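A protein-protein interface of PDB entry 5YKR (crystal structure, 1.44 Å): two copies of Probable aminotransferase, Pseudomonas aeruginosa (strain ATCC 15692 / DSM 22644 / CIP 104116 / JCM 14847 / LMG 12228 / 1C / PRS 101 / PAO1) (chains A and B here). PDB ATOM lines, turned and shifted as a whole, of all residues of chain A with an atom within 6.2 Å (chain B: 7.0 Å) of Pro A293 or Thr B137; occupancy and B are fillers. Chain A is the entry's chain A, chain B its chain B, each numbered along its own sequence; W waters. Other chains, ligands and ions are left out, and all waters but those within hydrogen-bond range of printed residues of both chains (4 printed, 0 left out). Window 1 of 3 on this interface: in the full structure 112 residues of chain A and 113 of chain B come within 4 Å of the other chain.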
ATOM      1  N   THR A 136      12.030   0.274  13.457  1.00  0.00           N
ATOM      2  CA  THR A 136      10.676   0.797  13.685  1.00  0.00           C
ATOM      3  C   THR A 136       9.706   0.257  12.612  1.00  0.00           C
ATOM      4  O   THR A 136      10.134  -0.440  11.676  1.00  0.00           O
ATOM      5  CB  THR A 136      10.652   2.314  13.687  1.00  0.00           C
ATOM      6  OG1 THR A 136      10.963   2.743  12.361  1.00  0.00           O
ATOM      7  CG2 THR A 136      11.582   2.920  14.725  1.00  0.00           C
ATOM      8  N   THR A 137       8.442   0.669  12.679  1.00  0.00           N
ATOM      9  CA  THR A 137       7.470   0.318  11.606  1.00  0.00           C
ATOM     10  C   THR A 137       7.324   1.382  10.541  1.00  0.00           C
ATOM     11  O   THR A 137       6.525   1.190   9.627  1.00  0.00           O
ATOM     12  CB  THR A 137       6.117  -0.091  12.221  1.00  0.00           C
ATOM     13  OG1 THR A 137       5.607   0.953  13.019  1.00  0.00           O
ATOM     14  CG2 THR A 137       6.249  -1.329  13.065  1.00  0.00           C
ATOM     15  N   SER A 138       8.066   2.476  10.643  1.00  0.00           N
ATOM     16  CA  SER A 138       8.045   3.531   9.575  1.00  0.00           C
ATOM     17  C   SER A 138       9.188   4.518   9.766  1.00  0.00           C
ATOM     18  O   SER A 138       9.684   4.711  10.859  1.00  0.00           O
ATOM     19  CB  SER A 138       6.750   4.318   9.646  1.00  0.00           C
ATOM     20  OG  SER A 138       6.661   5.114  10.832  1.00  0.00           O
ATOM     21  N   ASP A 141       8.356   7.063  12.396  1.00  0.00           N
ATOM     22  CA  ASP A 141       8.605   6.680  13.772  1.00  0.00           C
ATOM     23  C   ASP A 141      10.094   6.715  14.102  1.00  0.00           C
ATOM     24  O   ASP A 141      10.474   7.092  15.203  1.00  0.00           O
ATOM     25  CB  ASP A 141       8.038   5.298  14.052  1.00  0.00           C
ATOM     26  CG  ASP A 141       6.555   5.294  14.234  1.00  0.00           C
ATOM     27  OD1 ASP A 141       5.899   6.372  14.198  1.00  0.00           O
ATOM     28  OD2 ASP A 141       6.038   4.165  14.484  1.00  0.00           O
ATOM     29  N   ALA A 289      12.109  -3.433   3.266  1.00  0.00           N
ATOM     30  CA  ALA A 289      11.514  -4.671   3.762  1.00  0.00           C
ATOM     31  C   ALA A 289      10.383  -5.178   2.850  1.00  0.00           C
ATOM     32  O   ALA A 289       9.416  -5.743   3.280  1.00  0.00           O
ATOM     33  CB  ALA A 289      11.073  -4.581   5.209  1.00  0.00           C
ATOM     34  N   GLY A 291       7.964  -4.021   1.160  1.00  0.00           N
ATOM     35  CA  GLY A 291       6.597  -3.583   1.322  1.00  0.00           C
ATOM     36  C   GLY A 291       5.982  -3.875   2.675  1.00  0.00           C
ATOM     37  O   GLY A 291       4.840  -3.476   2.936  1.00  0.00           O
ATOM     38  N   ILE A 292       6.719  -4.536   3.578  1.00  0.00           N
ATOM     39  CA  ILE A 292       6.328  -4.584   4.977  1.00  0.00           C
ATOM     40  C   ILE A 292       6.718  -3.220   5.583  1.00  0.00           C
ATOM     41  O   ILE A 292       7.867  -2.761   5.442  1.00  0.00           O
ATOM     42  CB  ILE A 292       7.101  -5.676   5.721  1.00  0.00           C
ATOM     43  CG1 ILE A 292       6.841  -7.045   5.069  1.00  0.00           C
ATOM     44  CG2 ILE A 292       6.687  -5.729   7.197  1.00  0.00           C
ATOM     45  CD1 ILE A 292       7.778  -8.041   5.600  1.00  0.00           C
ATOM     46  N   PRO A 293       5.776  -2.554   6.260  1.00  0.00           N
ATOM     47  CA  PRO A 293       6.113  -1.275   6.920  1.00  0.00           C
ATOM     48  C   PRO A 293       7.304  -1.432   7.842  1.00  0.00           C
ATOM     49  O   PRO A 293       7.295  -2.264   8.753  1.00  0.00           O
ATOM     50  CB  PRO A 293       4.824  -0.940   7.691  1.00  0.00           C
ATOM     51  CG  PRO A 293       3.731  -1.574   6.850  1.00  0.00           C
ATOM     52  CD  PRO A 293       4.330  -2.870   6.361  1.00  0.00           C
ATOM     53  N   SER A 294       8.335  -0.623   7.621  1.00  0.00           N
ATOM     54  CA  SER A 294       9.602  -0.767   8.342  1.00  0.00           C
ATOM     55  C   SER A 294      10.473   0.450   8.153  1.00  0.00           C
ATOM     56  O   SER A 294      10.309   1.210   7.177  1.00  0.00           O
ATOM     57  CB  SER A 294      10.400  -1.976   7.848  1.00  0.00           C
ATOM     58  OG  SER A 294       9.703  -3.199   7.777  1.00  0.00           O
ATOM     59  N   ALA A 295      11.387   0.637   9.103  1.00  0.00           N
ATOM     60  CA  ALA A 295      12.524   1.527   8.912  1.00  0.00           C
ATOM     61  C   ALA A 295      13.620   1.077   9.866  1.00  0.00           C
ATOM     62  O   ALA A 295      13.353   0.359  10.852  1.00  0.00           O
ATOM     63  CB  ALA A 295      12.148   2.995   9.185  1.00  0.00           C
ATOM     64  N   LEU A 329       5.013  -4.282  16.937  1.00  0.00           N
ATOM     65  CA  LEU A 329       5.436  -5.043  15.800  1.00  0.00           C
ATOM     66  C   LEU A 329       6.757  -4.537  15.230  1.00  0.00           C
ATOM     67  O   LEU A 329       7.244  -5.024  14.206  1.00  0.00           O
ATOM     68  CB  LEU A 329       4.366  -5.145  14.724  1.00  0.00           C
ATOM     69  CG  LEU A 329       3.268  -6.167  15.035  1.00  0.00           C
ATOM     70  CD1 LEU A 329       2.327  -5.715  16.115  1.00  0.00           C
ATOM     71  CD2 LEU A 329       2.465  -6.543  13.805  1.00  0.00           C
ATOM     72  N   GLN A 335       9.889  -8.594   9.373  1.00  0.00           N
ATOM     73  CA  GLN A 335      10.665  -7.450   8.900  1.00  0.00           C
ATOM     74  C   GLN A 335      12.125  -7.802   8.718  1.00  0.00           C
ATOM     75  O   GLN A 335      12.742  -7.469   7.706  1.00  0.00           O
ATOM     76  CB  GLN A 335      10.615  -6.290   9.895  1.00  0.00           C
ATOM     77  CG  GLN A 335       9.274  -5.545  10.003  1.00  0.00           C
ATOM     78  CD  GLN A 335       9.424  -4.437  11.069  1.00  0.00           C
ATOM     79  OE1 GLN A 335       9.998  -4.693  12.151  1.00  0.00           O
ATOM     80  NE2 GLN A 335       9.007  -3.226  10.769  1.00  0.00           N
ATOM     81  N   VAL B 135      -6.752   2.799   7.058  1.00  0.00           N
ATOM     82  CA  VAL B 135      -5.685   1.879   7.523  1.00  0.00           C
ATOM     83  C   VAL B 135      -4.432   2.683   7.847  1.00  0.00           C
ATOM     84  O   VAL B 135      -4.064   3.605   7.092  1.00  0.00           O
ATOM     85  CB  VAL B 135      -5.381   0.836   6.475  1.00  0.00           C
ATOM     86  CG1 VAL B 135      -4.282  -0.119   6.895  1.00  0.00           C
ATOM     87  CG2 VAL B 135      -6.645   0.079   6.107  1.00  0.00           C
ATOM     88  N   THR B 136      -3.744   2.269   8.907  1.00  0.00           N
ATOM     89  CA  THR B 136      -2.438   2.850   9.290  1.00  0.00           C
ATOM     90  C   THR B 136      -1.405   1.706   9.437  1.00  0.00           C
ATOM     91  O   THR B 136      -1.751   0.515   9.251  1.00  0.00           O
ATOM     92  CB  THR B 136      -2.510   3.606  10.605  1.00  0.00           C
ATOM     93  OG1 THR B 136      -2.774   2.655  11.632  1.00  0.00           O
ATOM     94  CG2 THR B 136      -3.551   4.731  10.579  1.00  0.00           C
ATOM     95  N   THR B 137      -0.162   2.040   9.764  1.00  0.00           N
ATOM     96  CA  THR B 137       0.868   1.011  10.031  1.00  0.00           C
ATOM     97  C   THR B 137       0.993   0.627  11.482  1.00  0.00           C
ATOM     98  O   THR B 137       1.817  -0.230  11.808  1.00  0.00           O
ATOM     99  CB  THR B 137       2.212   1.406   9.415  1.00  0.00           C
ATOM    100  OG1 THR B 137       2.631   2.667   9.913  1.00  0.00           O
ATOM    101  CG2 THR B 137       2.112   1.475   7.906  1.00  0.00           C
ATOM    102  N   SER B 138       0.170   1.212  12.366  1.00  0.00           N
ATOM    103  CA  SER B 138       0.193   0.834  13.797  1.00  0.00           C
ATOM    104  C   SER B 138      -1.013   1.395  14.537  1.00  0.00           C
ATOM    105  O   SER B 138      -1.570   2.434  14.144  1.00  0.00           O
ATOM    106  CB  SER B 138       1.434   1.367  14.490  1.00  0.00           C
ATOM    107  OG  SER B 138       1.413   2.773  14.588  1.00  0.00           O
ATOM    108  N   ALA B 139      -1.365   0.753  15.653  1.00  0.00           N
ATOM    109  CA  ALA B 139      -2.411   1.302  16.521  1.00  0.00           C
ATOM    110  C   ALA B 139      -2.035   2.707  17.034  1.00  0.00           C
ATOM    111  O   ALA B 139      -2.894   3.580  17.088  1.00  0.00           O
ATOM    112  CB  ALA B 139      -2.686   0.407  17.690  1.00  0.00           C
ATOM    113  N   THR B 140      -0.771   2.901  17.349  1.00  0.00           N
ATOM    114  CA  THR B 140      -0.311   4.254  17.738  1.00  0.00           C
ATOM    115  C   THR B 140      -0.739   5.275  16.694  1.00  0.00           C
ATOM    116  O   THR B 140      -1.296   6.327  17.029  1.00  0.00           O
ATOM    117  CB  THR B 140       1.182   4.286  17.931  1.00  0.00           C
ATOM    118  OG1 THR B 140       1.556   3.529  19.064  1.00  0.00           O
ATOM    119  CG2 THR B 140       1.645   5.711  18.152  1.00  0.00           C
ATOM    120  N   ASP B 141      -0.412   4.992  15.438  1.00  0.00           N
ATOM    121  CA  ASP B 141      -0.714   5.956  14.393  1.00  0.00           C
ATOM    122  C   ASP B 141      -2.209   6.188  14.229  1.00  0.00           C
ATOM    123  O   ASP B 141      -2.646   7.306  13.967  1.00  0.00           O
ATOM    124  CB  ASP B 141      -0.097   5.558  13.086  1.00  0.00           C
ATOM    125  CG  ASP B 141       1.393   5.787  13.016  1.00  0.00           C
ATOM    126  OD1 ASP B 141       1.991   6.344  13.985  1.00  0.00           O
ATOM    127  OD2 ASP B 141       1.948   5.474  11.926  1.00  0.00           O
ATOM    128  N   ALA B 142      -3.005   5.111  14.328  1.00  0.00           N
ATOM    129  CA  ALA B 142      -4.455   5.302  14.279  1.00  0.00           C
ATOM    130  C   ALA B 142      -4.892   6.269  15.357  1.00  0.00           C
ATOM    131  O   ALA B 142      -5.670   7.196  15.107  1.00  0.00           O
ATOM    132  CB  ALA B 142      -5.178   3.945  14.355  1.00  0.00           C
ATOM    133  N   PHE B 145      -3.672   9.927  14.552  1.00  0.00           N
ATOM    134  CA  PHE B 145      -4.328  10.526  13.375  1.00  0.00           C
ATOM    135  C   PHE B 145      -5.777  10.852  13.700  1.00  0.00           C
ATOM    136  O   PHE B 145      -6.261  11.919  13.323  1.00  0.00           O
ATOM    137  CB  PHE B 145      -4.240   9.621  12.166  1.00  0.00           C
ATOM    138  CG  PHE B 145      -2.815   9.307  11.704  1.00  0.00           C
ATOM    139  CD1 PHE B 145      -1.730  10.050  12.095  1.00  0.00           C
ATOM    140  CD2 PHE B 145      -2.633   8.287  10.807  1.00  0.00           C
ATOM    141  CE1 PHE B 145      -0.449   9.744  11.663  1.00  0.00           C
ATOM    142  CE2 PHE B 145      -1.352   7.965  10.350  1.00  0.00           C
ATOM    143  CZ  PHE B 145      -0.265   8.717  10.777  1.00  0.00           C
ATOM    144  N1  LLP B 286      -3.460   0.719  22.242  1.00  0.00           N
ATOM    145  C2  LLP B 286      -3.552  -0.302  23.091  1.00  0.00           C
ATOM    146  C2' LLP B 286      -4.755  -0.404  23.990  1.00  0.00           C
ATOM    147  C3  LLP B 286      -2.495  -1.300  23.076  1.00  0.00           C
ATOM    148  O3  LLP B 286      -2.591  -2.346  23.897  1.00  0.00           O
ATOM    149  C4  LLP B 286      -1.391  -1.194  22.148  1.00  0.00           C
ATOM    150  C4' LLP B 286      -0.314  -2.189  21.964  1.00  0.00           C
ATOM    151  C5  LLP B 286      -1.350   0.011  21.348  1.00  0.00           C
ATOM    152  C6  LLP B 286      -2.414   0.930  21.432  1.00  0.00           C
ATOM    153  C5' LLP B 286      -0.186   0.402  20.475  1.00  0.00           C
ATOM    154  OP4 LLP B 286       0.121  -0.549  19.477  1.00  0.00           O
ATOM    155  P   LLP B 286       1.511  -0.360  18.666  1.00  0.00           P
ATOM    156  OP1 LLP B 286       1.453  -1.520  17.682  1.00  0.00           O
ATOM    157  OP2 LLP B 286       2.655  -0.585  19.643  1.00  0.00           O
ATOM    158  OP3 LLP B 286       1.447   1.031  18.043  1.00  0.00           O
ATOM    159  N   LLP B 286      -2.326  -4.144  16.351  1.00  0.00           N
ATOM    160  CA  LLP B 286      -1.583  -5.359  16.774  1.00  0.00           C
ATOM    161  CB  LLP B 286      -1.713  -5.708  18.266  1.00  0.00           C
ATOM    162  CG  LLP B 286      -0.884  -4.826  19.267  1.00  0.00           C
ATOM    163  CD  LLP B 286      -0.814  -5.405  20.707  1.00  0.00           C
ATOM    164  CE  LLP B 286      -0.008  -4.662  21.860  1.00  0.00           C
ATOM    165  NZ  LLP B 286      -0.699  -3.488  22.396  1.00  0.00           N
ATOM    166  C   LLP B 286      -1.804  -6.622  15.937  1.00  0.00           C
ATOM    167  O   LLP B 286      -0.871  -7.101  15.305  1.00  0.00           O
ATOM    168  N   ILE B 292       2.226  -8.325   9.832  1.00  0.00           N
ATOM    169  CA  ILE B 292       2.533  -7.101   9.096  1.00  0.00           C
ATOM    170  C   ILE B 292       2.042  -5.923   9.940  1.00  0.00           C
ATOM    171  O   ILE B 292       0.874  -5.889  10.329  1.00  0.00           O
ATOM    172  CB  ILE B 292       1.778  -7.064   7.753  1.00  0.00           C
ATOM    173  CG1 ILE B 292       2.176  -8.337   6.944  1.00  0.00           C
ATOM    174  CG2 ILE B 292       2.103  -5.811   6.959  1.00  0.00           C
ATOM    175  CD1 ILE B 292       1.353  -8.490   5.820  1.00  0.00           C
ATOM    176  N   PRO B 293       2.918  -4.931  10.225  1.00  0.00           N
ATOM    177  CA  PRO B 293       2.490  -3.774  11.034  1.00  0.00           C
ATOM    178  C   PRO B 293       1.266  -3.113  10.394  1.00  0.00           C
ATOM    179  O   PRO B 293       1.308  -2.719   9.215  1.00  0.00           O
ATOM    180  CB  PRO B 293       3.703  -2.887  11.017  1.00  0.00           C
ATOM    181  CG  PRO B 293       4.867  -3.831  10.862  1.00  0.00           C
ATOM    182  CD  PRO B 293       4.359  -4.901   9.913  1.00  0.00           C
ATOM    183  N   SER B 294       0.189  -2.977  11.150  1.00  0.00           N
ATOM    184  CA  SER B 294      -1.065  -2.495  10.644  1.00  0.00           C
ATOM    185  C   SER B 294      -2.022  -2.127  11.760  1.00  0.00           C
ATOM    186  O   SER B 294      -1.991  -2.744  12.852  1.00  0.00           O
ATOM    187  CB  SER B 294      -1.777  -3.559   9.825  1.00  0.00           C
ATOM    188  OG  SER B 294      -1.016  -4.190   8.838  1.00  0.00           O
ATOM    189  N   ALA B 295      -2.977  -1.256  11.421  1.00  0.00           N
ATOM    190  CA  ALA B 295      -4.134  -1.022  12.257  1.00  0.00           C
ATOM    191  C   ALA B 295      -5.245  -0.468  11.364  1.00  0.00           C
ATOM    192  O   ALA B 295      -4.975   0.012  10.244  1.00  0.00           O
ATOM    193  CB  ALA B 295      -3.849  -0.033  13.387  1.00  0.00           C
ATOM    194  N   GLY B 327       0.560   7.569   5.836  1.00  0.00           N
ATOM    195  CA  GLY B 327       1.930   7.129   5.751  1.00  0.00           C
ATOM    196  C   GLY B 327       2.151   6.315   4.489  1.00  0.00           C
ATOM    197  O   GLY B 327       1.192   5.783   3.898  1.00  0.00           O
ATOM    198  N   THR B 328       3.411   6.241   4.044  1.00  0.00           N
ATOM    199  CA  THR B 328       3.665   5.771   2.678  1.00  0.00           C
ATOM    200  C   THR B 328       3.244   4.317   2.438  1.00  0.00           C
ATOM    201  O   THR B 328       2.795   3.968   1.342  1.00  0.00           O
ATOM    202  CB  THR B 328       5.129   6.016   2.323  1.00  0.00           C
ATOM    203  OG1 THR B 328       5.465   7.391   2.574  1.00  0.00           O
ATOM    204  CG2 THR B 328       5.394   5.661   0.840  1.00  0.00           C
ATOM    205  N   LEU B 329       3.420   3.479   3.464  1.00  0.00           N
ATOM    206  CA  LEU B 329       3.053   2.058   3.335  1.00  0.00           C
ATOM    207  C   LEU B 329       1.745   1.755   4.036  1.00  0.00           C
ATOM    208  O   LEU B 329       1.331   0.579   4.097  1.00  0.00           O
ATOM    209  CB  LEU B 329       4.171   1.162   3.854  1.00  0.00           C
ATOM    210  CG  LEU B 329       5.341   0.998   2.855  1.00  0.00           C
ATOM    211  CD1 LEU B 329       6.219   2.212   2.697  1.00  0.00           C
ATOM    212  CD2 LEU B 329       6.206  -0.166   3.221  1.00  0.00           C
ATOM    213  N   ALA B 330       1.025   2.785   4.476  1.00  0.00           N
ATOM    214  CA  ALA B 330      -0.293   2.542   5.070  1.00  0.00           C
ATOM    215  C   ALA B 330      -1.329   2.151   4.019  1.00  0.00           C
ATOM    216  O   ALA B 330      -1.415   2.751   2.958  1.00  0.00           O
ATOM    217  CB  ALA B 330      -0.753   3.776   5.812  1.00  0.00           C
ATOM    218  N   GLY B 331      -2.187   1.186   4.360  1.00  0.00           N
ATOM    219  CA  GLY B 331      -3.215   0.733   3.466  1.00  0.00           C
ATOM    220  C   GLY B 331      -2.707  -0.013   2.261  1.00  0.00           C
ATOM    221  O   GLY B 331      -3.358   0.038   1.212  1.00  0.00           O
ATOM    222  N   ASN B 332      -1.533  -0.663   2.354  1.00  0.00           N
ATOM    223  CA  ASN B 332      -0.946  -1.300   1.201  1.00  0.00           C
ATOM    224  C   ASN B 332      -1.518  -2.664   0.852  1.00  0.00           C
ATOM    225  O   ASN B 332      -2.233  -3.277   1.654  1.00  0.00           O
ATOM    226  CB  ASN B 332       0.581  -1.238   1.214  1.00  0.00           C
ATOM    227  CG  ASN B 332       1.273  -2.233   2.109  1.00  0.00           C
ATOM    228  OD1 ASN B 332       0.712  -3.239   2.564  1.00  0.00           O
ATOM    229  ND2 ASN B 332       2.587  -1.981   2.295  1.00  0.00           N
ATOM    230  N   LEU B 334      -0.237  -5.609   0.657  1.00  0.00           N
ATOM    231  CA  LEU B 334       0.156  -6.705   1.549  1.00  0.00           C
ATOM    232  C   LEU B 334      -0.670  -6.698   2.851  1.00  0.00           C
ATOM    233  O   LEU B 334      -1.207  -7.766   3.259  1.00  0.00           O
ATOM    234  CB  LEU B 334       1.648  -6.588   1.824  1.00  0.00           C
ATOM    235  CG  LEU B 334       2.287  -7.792   2.465  1.00  0.00           C
ATOM    236  CD1 LEU B 334       2.232  -8.985   1.524  1.00  0.00           C
ATOM    237  CD2 LEU B 334       3.732  -7.468   2.829  1.00  0.00           C
ATOM    238  N   GLN B 335      -0.837  -5.510   3.447  1.00  0.00           N
ATOM    239  CA  GLN B 335      -1.685  -5.428   4.640  1.00  0.00           C
ATOM    240  C   GLN B 335      -3.097  -5.882   4.345  1.00  0.00           C
ATOM    241  O   GLN B 335      -3.707  -6.609   5.123  1.00  0.00           O
ATOM    242  CB  GLN B 335      -1.763  -3.978   5.114  1.00  0.00           C
ATOM    243  CG  GLN B 335      -0.489  -3.356   5.731  1.00  0.00           C
ATOM    244  CD  GLN B 335      -0.773  -1.924   6.126  1.00  0.00           C
ATOM    245  OE1 GLN B 335      -1.393  -1.192   5.344  1.00  0.00           O
ATOM    246  NE2 GLN B 335      -0.428  -1.536   7.342  1.00  0.00           N
HETATM  247  O   HOH W   1       3.565   4.374  15.264  1.00  0.00           O
HETATM  248  O   HOH W   2       3.570  -1.895  16.069  1.00  0.00           O
HETATM  249  O   HOH W   3       4.393   6.364  11.802  1.00  0.00           O
HETATM  250  O   HOH W   4       4.047   2.966  12.154  1.00  0.00           O
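Of the printed residues of chain B, Gly A291 touches Leu B329 (3.6 Å) and Asn B332 (2.8 Å).
Of chain B, only Thr B137, Ile B292, Pro B293 and Leu B329 come within 4 Å of Pro A293.
Of the printed residues of chain B, Leu A329 touches LLP B286 (3.6 Å), Ile B292 (3.9 Å) and Pro B293 (3.9 Å).
Gln A335 touches none of the printed residues of chain B.
Printed residues of chain A within 4 Å of Thr B137: Pro A293 (3.6 Å).
Printed residues of chain A within 4 Å of Ile B292: Pro A293 and Leu A329.
Ser B294 touches none of the printed residues of chain A.
Of the printed residues of chain A, Asn B332 touches Gly A291 (2.8 Å).
The nearest residue of chain B that does not touch Pro A293 is Gln B335 (4.2 Å).
The nearest printed residue of chain A that does not touch Leu B329 is Ser A294 (4.9 Å).
O of Leu A329 sits close to OE1 of Gln A335, at 3.5 Å.
The side-chain hydroxyl (OG) of Ser A138 sits at hydrogen-bond distance from the backbone NH (N) of Asp A141 (3.0 Å).
The backbone NH (N) of Asp B141 lies within hydrogen-bond range of the side-chain hydroxyl (OG) of Ser B138 (3.0 Å).
The backbone NH of Ser A294 sits at hydrogen-bond distance from the backbone carbonyl oxygen of Thr A137, at 3.3 Å.
The backbone carbonyl oxygen of Pro B293 lies within hydrogen-bond range of the side-chain amide nitrogen of Gln B335 (2.8 Å).
The side-chain amide nitrogen (ND2) of Asn B332 sits at hydrogen-bond distance from the backbone carbonyl oxygen (O) of Leu B329.
Thr A137 touches Pro B293.
Asp A141 touches Asp B141 (OD1 to OD1, 3.9 Å).
Ile A292 touches Pro B293.
O of Ile A292 touches CD2 of Leu B329, 3.8 Å away.
Pro A293 touches Ile B292 (CD to CG2, 3.7 Å).
Pro A293 touches Pro B293 (CG to O, 3.6 Å).
Pro A293 touches Leu B329 (CA to CD2, 3.9 Å).
CD1 of Leu A329 touches O of LLP B286, at 3.6 Å.
CD2 of Leu A329 touches O of Ile B292 (3.9 Å).
Pro B293 touches Leu A329.
Asp B141 touches its own counterpart, Asp A141.
Ile A292 touches Pro B293, and with the chains exchanged Pro A293 touches Ile B292.
Ile A292 touches Leu B329, and with the chains exchanged Leu A329 touches Ile B292.
Pro A293 touches Leu B329, and with the chains exchanged Leu A329 touches Pro B293.
O of Gly A291 is in hydrogen-bond range of ND2 of Asn B332 (2.8 Å).
Water W1 lies within hydrogen-bond range of OD2 of Asp A141 (2.6 Å), OG of Ser B138 (2.8 Å) and OD1 of Asp B141 (2.8 Å).
Water W3 lies within hydrogen-bond range of OD2 of Asp B141 (2.6 Å), OG of Ser A138 (2.8 Å) and OD1 of Asp A141 (2.8 Å).
Water W4 lies within hydrogen-bond range of OG1 of Thr B137 (2.7 Å), OG1 of Thr A137 (2.7 Å), OD2 of Asp B141 (3.3 Å) and OD2 of Asp A141 (3.3 Å).
Water W2 lies within hydrogen-bond range of OP1 of LLP B286 (2.7 Å) and the backbone NH of Leu A329 (2.9 Å).
Printed residues of chain B that touch a printed residue of chain A: Thr B137, Asp B141, LLP B286, Ile B292, Pro B293, Leu B329, Asn B332 and Leu B334.
Hydrophobic or aromatic side chains of chain B within 4 Å of the printed part of chain A: Ile B292, Pro B293, Leu B329 and Leu B334.
Printed residues of chain A that touch a printed residue of chain B: Thr A137, Asp A141, Gly A291, Ile A292, Pro A293 and Leu A329.
Hydrophobic or aromatic side chains of chain A that line the printed part of chain B: Ile A292, Pro A293 and Leu A329.
Along chain A the printed residues that touch a printed residue of chain B span positions 137 to 329.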
